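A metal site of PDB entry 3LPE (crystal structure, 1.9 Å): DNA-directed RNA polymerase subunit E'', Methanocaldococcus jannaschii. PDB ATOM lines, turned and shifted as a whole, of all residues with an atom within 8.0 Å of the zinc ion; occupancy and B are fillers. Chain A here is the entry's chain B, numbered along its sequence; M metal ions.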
ATOM      1  N   ALA A   3       6.007  11.647  26.227  1.00  0.00           N
ATOM      2  CA  ALA A   3       4.931  11.342  25.296  1.00  0.00           C
ATOM      3  C   ALA A   3       5.152  12.143  24.027  1.00  0.00           C
ATOM      4  O   ALA A   3       5.524  13.318  24.093  1.00  0.00           O
ATOM      5  CB  ALA A   3       3.570  11.673  25.911  1.00  0.00           C
ATOM      6  N   CYS A   4       4.922  11.522  22.878  1.00  0.00           N
ATOM      7  CA  CYS A   4       4.993  12.243  21.609  1.00  0.00           C
ATOM      8  C   CYS A   4       4.070  13.439  21.594  1.00  0.00           C
ATOM      9  O   CYS A   4       2.908  13.318  21.925  1.00  0.00           O
ATOM     10  CB  CYS A   4       4.629  11.301  20.431  1.00  0.00           C
ATOM     11  SG  CYS A   4       4.742  12.202  18.872  1.00  0.00           S
ATOM     12  N   LEU A   5       4.578  14.610  21.194  1.00  0.00           N
ATOM     13  CA  LEU A   5       3.748  15.820  21.151  1.00  0.00           C
ATOM     14  C   LEU A   5       2.635  15.730  20.104  1.00  0.00           C
ATOM     15  O   LEU A   5       1.635  16.424  20.204  1.00  0.00           O
ATOM     16  CB  LEU A   5       4.617  17.056  20.861  1.00  0.00           C
ATOM     17  CG  LEU A   5       5.530  17.507  22.005  1.00  0.00           C
ATOM     18  CD1 LEU A   5       6.629  18.433  21.494  1.00  0.00           C
ATOM     19  CD2 LEU A   5       4.725  18.164  23.133  1.00  0.00           C
ATOM     20  N   LYS A   6       2.812  14.860  19.113  1.00  0.00           N
ATOM     21  CA  LYS A   6       1.837  14.731  18.030  1.00  0.00           C
ATOM     22  C   LYS A   6       0.859  13.573  18.226  1.00  0.00           C
ATOM     23  O   LYS A   6      -0.344  13.753  18.101  1.00  0.00           O
ATOM     24  CB  LYS A   6       2.584  14.566  16.689  1.00  0.00           C
ATOM     25  CG  LYS A   6       1.762  14.939  15.475  1.00  0.00           C
ATOM     26  CD  LYS A   6       2.558  14.738  14.163  1.00  0.00           C
ATOM     27  CE  LYS A   6       3.799  15.622  14.103  1.00  0.00           C
ATOM     28  NZ  LYS A   6       4.370  15.710  12.723  1.00  0.00           N
ATOM     29  N   CYS A   7       1.379  12.382  18.516  1.00  0.00           N
ATOM     30  CA  CYS A   7       0.536  11.194  18.568  1.00  0.00           C
ATOM     31  C   CYS A   7       0.448  10.622  19.973  1.00  0.00           C
ATOM     32  O   CYS A   7      -0.250   9.655  20.186  1.00  0.00           O
ATOM     33  CB  CYS A   7       1.008  10.111  17.587  1.00  0.00           C
ATOM     34  SG  CYS A   7       2.459   9.106  18.093  1.00  0.00           S
ATOM     35  N   LYS A   8       1.157  11.235  20.917  1.00  0.00           N
ATOM     36  CA  LYS A   8       0.993  10.876  22.357  1.00  0.00           C
ATOM     37  C   LYS A   8       1.569   9.519  22.764  1.00  0.00           C
ATOM     38  O   LYS A   8       1.452   9.091  23.926  1.00  0.00           O
ATOM     39  CB  LYS A   8      -0.484  11.007  22.789  1.00  0.00           C
ATOM     40  CG  LYS A   8      -0.994  12.428  22.705  1.00  0.00           C
ATOM     41  CD  LYS A   8      -2.440  12.586  23.200  1.00  0.00           C
ATOM     42  CE  LYS A   8      -3.434  12.151  22.140  1.00  0.00           C
ATOM     43  NZ  LYS A   8      -4.762  12.808  22.351  1.00  0.00           N
ATOM     44  N   TYR A   9       2.228   8.841  21.822  1.00  0.00           N
ATOM     45  CA  TYR A   9       2.909   7.599  22.147  1.00  0.00           C
ATOM     46  C   TYR A   9       3.901   7.802  23.298  1.00  0.00           C
ATOM     47  O   TYR A   9       4.679   8.777  23.310  1.00  0.00           O
ATOM     48  CB  TYR A   9       3.668   7.091  20.929  1.00  0.00           C
ATOM     49  CG  TYR A   9       4.277   5.722  21.072  1.00  0.00           C
ATOM     50  CD1 TYR A   9       3.527   4.574  20.869  1.00  0.00           C
ATOM     51  CD2 TYR A   9       5.632   5.577  21.324  1.00  0.00           C
ATOM     52  CE1 TYR A   9       4.114   3.304  20.961  1.00  0.00           C
ATOM     53  CE2 TYR A   9       6.231   4.327  21.424  1.00  0.00           C
ATOM     54  CZ  TYR A   9       5.469   3.195  21.236  1.00  0.00           C
ATOM     55  OH  TYR A   9       6.077   1.959  21.313  1.00  0.00           O
ATOM     56  N   LEU A  10       3.885   6.874  24.242  1.00  0.00           N
ATOM     57  CA  LEU A  10       4.745   7.020  25.423  1.00  0.00           C
ATOM     58  C   LEU A  10       6.058   6.305  25.267  1.00  0.00           C
ATOM     59  O   LEU A  10       6.078   5.146  24.866  1.00  0.00           O
ATOM     60  CB  LEU A  10       4.022   6.451  26.645  1.00  0.00           C
ATOM     61  CG  LEU A  10       2.781   7.236  27.061  1.00  0.00           C
ATOM     62  CD1 LEU A  10       2.127   6.443  28.186  1.00  0.00           C
ATOM     63  CD2 LEU A  10       3.203   8.582  27.588  1.00  0.00           C
ATOM     64  N   THR A  11       7.143   6.995  25.605  1.00  0.00           N
ATOM     65  CA  THR A  11       8.499   6.460  25.453  1.00  0.00           C
ATOM     66  C   THR A  11       9.530   7.246  26.281  1.00  0.00           C
ATOM     67  O   THR A  11       9.332   8.420  26.610  1.00  0.00           O
ATOM     68  CB  THR A  11       8.932   6.442  23.966  1.00  0.00           C
ATOM     69  OG1 THR A  11      10.254   5.903  23.861  1.00  0.00           O
ATOM     70  CG2 THR A  11       8.918   7.830  23.381  1.00  0.00           C
ATOM     71  N   ILE A  15      12.471  11.266  20.930  1.00  0.00           N
ATOM     72  CA  ILE A  15      11.898  11.335  19.594  1.00  0.00           C
ATOM     73  C   ILE A  15      10.965  10.141  19.418  1.00  0.00           C
ATOM     74  O   ILE A  15      11.325   9.033  19.780  1.00  0.00           O
ATOM     75  CB  ILE A  15      12.998  11.279  18.507  1.00  0.00           C
ATOM     76  CG1 ILE A  15      13.863  12.531  18.537  1.00  0.00           C
ATOM     77  CG2 ILE A  15      12.382  11.072  17.107  1.00  0.00           C
ATOM     78  CD1 ILE A  15      15.020  12.475  17.514  1.00  0.00           C
ATOM     79  N   CYS A  16       9.771  10.377  18.881  1.00  0.00           N
ATOM     80  CA  CYS A  16       8.760   9.349  18.762  1.00  0.00           C
ATOM     81  C   CYS A  16       9.153   8.324  17.718  1.00  0.00           C
ATOM     82  O   CYS A  16       9.481   8.688  16.585  1.00  0.00           O
ATOM     83  CB  CYS A  16       7.425   9.968  18.391  1.00  0.00           C
ATOM     84  SG  CYS A  16       6.079   8.783  18.202  1.00  0.00           S
ATOM     85  N   PRO A  17       9.125   7.045  18.087  1.00  0.00           N
ATOM     86  CA  PRO A  17       9.503   5.947  17.175  1.00  0.00           C
ATOM     87  C   PRO A  17       8.472   5.761  16.065  1.00  0.00           C
ATOM     88  O   PRO A  17       8.745   5.132  15.031  1.00  0.00           O
ATOM     89  CB  PRO A  17       9.535   4.706  18.084  1.00  0.00           C
ATOM     90  CG  PRO A  17       9.409   5.212  19.485  1.00  0.00           C
ATOM     91  CD  PRO A  17       8.754   6.556  19.423  1.00  0.00           C
ATOM     92  N   ILE A  18       7.272   6.291  16.261  1.00  0.00           N
ATOM     93  CA  ILE A  18       6.247   6.195  15.233  1.00  0.00           C
ATOM     94  C   ILE A  18       6.348   7.306  14.206  1.00  0.00           C
ATOM     95  O   ILE A  18       6.475   7.044  13.015  1.00  0.00           O
ATOM     96  CB  ILE A  18       4.819   6.193  15.836  1.00  0.00           C
ATOM     97  CG1 ILE A  18       4.642   5.009  16.782  1.00  0.00           C
ATOM     98  CG2 ILE A  18       3.768   6.126  14.722  1.00  0.00           C
ATOM     99  CD1 ILE A  18       3.289   4.979  17.481  1.00  0.00           C
ATOM    100  N   CYS A  19       6.307   8.557  14.673  1.00  0.00           N
ATOM    101  CA  CYS A  19       6.119   9.700  13.779  1.00  0.00           C
ATOM    102  C   CYS A  19       7.281  10.711  13.786  1.00  0.00           C
ATOM    103  O   CYS A  19       7.230  11.752  13.105  1.00  0.00           O
ATOM    104  CB  CYS A  19       4.786  10.399  14.083  1.00  0.00           C
ATOM    105  SG  CYS A  19       4.834  11.442  15.591  1.00  0.00           S
ATOM    106  N   HIS A  20       8.336  10.405  14.535  1.00  0.00           N
ATOM    107  CA  HIS A  20       9.558  11.211  14.533  1.00  0.00           C
ATOM    108  C   HIS A  20       9.443  12.592  15.183  1.00  0.00           C
ATOM    109  O   HIS A  20      10.365  13.393  15.122  1.00  0.00           O
ATOM    110  CB  HIS A  20      10.133  11.322  13.116  1.00  0.00           C
ATOM    111  CG  HIS A  20      10.056  10.045  12.347  1.00  0.00           C
ATOM    112  ND1 HIS A  20       9.078   9.810  11.408  1.00  0.00           N
ATOM    113  CD2 HIS A  20      10.803   8.919  12.403  1.00  0.00           C
ATOM    114  CE1 HIS A  20       9.239   8.596  10.903  1.00  0.00           C
ATOM    115  NE2 HIS A  20      10.279   8.040  11.492  1.00  0.00           N
ATOM    116  N   SER A  21       8.311  12.884  15.813  1.00  0.00           N
ATOM    117  CA  SER A  21       8.171  14.201  16.432  1.00  0.00           C
ATOM    118  C   SER A  21       8.847  14.203  17.823  1.00  0.00           C
ATOM    119  O   SER A  21       9.152  13.158  18.368  1.00  0.00           O
ATOM    120  CB  SER A  21       6.705  14.613  16.478  1.00  0.00           C
ATOM    121  OG  SER A  21       6.170  14.512  17.785  1.00  0.00           O
ATOM    122  N   PRO A  22       9.120  15.389  18.372  1.00  0.00           N
ATOM    123  CA  PRO A  22       9.688  15.492  19.725  1.00  0.00           C
ATOM    124  C   PRO A  22       8.721  14.929  20.758  1.00  0.00           C
ATOM    125  O   PRO A  22       7.536  14.947  20.532  1.00  0.00           O
ATOM    126  CB  PRO A  22       9.825  17.013  19.927  1.00  0.00           C
ATOM    127  CG  PRO A  22       9.789  17.604  18.575  1.00  0.00           C
ATOM    128  CD  PRO A  22       8.930  16.713  17.736  1.00  0.00           C
ATOM    129  N   THR A  23       9.240  14.441  21.887  1.00  0.00           N
ATOM    130  CA  THR A  23       8.401  13.951  22.959  1.00  0.00           C
ATOM    131  C   THR A  23       8.548  14.900  24.133  1.00  0.00           C
ATOM    132  O   THR A  23       9.496  15.683  24.165  1.00  0.00           O
ATOM    133  CB  THR A  23       8.851  12.564  23.433  1.00  0.00           C
ATOM    134  OG1 THR A  23      10.166  12.629  23.991  1.00  0.00           O
ATOM    135  CG2 THR A  23       8.842  11.586  22.274  1.00  0.00           C
ATOM    136  N   TYR A  53      -0.205   5.228  25.401  1.00  0.00           N
ATOM    137  CA  TYR A  53      -0.376   6.604  24.977  1.00  0.00           C
ATOM    138  C   TYR A  53      -0.859   7.491  26.112  1.00  0.00           C
ATOM    139  O   TYR A  53      -1.645   7.061  26.979  1.00  0.00           O
ATOM    140  CB  TYR A  53      -1.430   6.683  23.856  1.00  0.00           C
ATOM    141  CG  TYR A  53      -1.038   5.911  22.620  1.00  0.00           C
ATOM    142  CD1 TYR A  53      -0.490   6.568  21.529  1.00  0.00           C
ATOM    143  CD2 TYR A  53      -1.222   4.544  22.548  1.00  0.00           C
ATOM    144  CE1 TYR A  53      -0.125   5.859  20.366  1.00  0.00           C
ATOM    145  CE2 TYR A  53      -0.864   3.830  21.406  1.00  0.00           C
ATOM    146  CZ  TYR A  53      -0.315   4.500  20.323  1.00  0.00           C
ATOM    147  OH  TYR A  53       0.041   3.801  19.198  1.00  0.00           O
HETATM  148 ZN    ZN M   1       4.386  10.271  17.584  1.00  0.00          ZN
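The side-chain hydroxyl of Ser 21 lies close to the side-chain sulfur of Cys 4, at 2.9 Å.
The side-chain sulfur of Cys 19 sits close to the backbone NH of Ser 21, at 3.8 Å.
The side-chain sulfur (SG) of Cys 7 lies close to the backbone NH (N) of Tyr 9 (3.7 Å).
The backbone NH (N) of Ile 18 sits close to the side-chain sulfur (SG) of Cys 16 (3.4 Å).
N of Cys 16 lies within hydrogen-bond range of O of Ser 21, 2.9 Å away.
N of Lys 6 sits close to SG of Cys 4, at 3.3 Å.
The backbone NH (N) of Cys 4 is in hydrogen-bond range of the backbone carbonyl oxygen (O) of Tyr 9 (2.8 Å).
Of the 19 residues printed, 4 come within 4 Å of the zinc ion.
The zinc ion is bound by the side-chain sulfur of Cys 7, the side-chain sulfur of Cys 16, the side-chain sulfur of Cys 4 and the side-chain sulfur of Cys 19.
The zinc ion has four donor atoms within binding distance.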
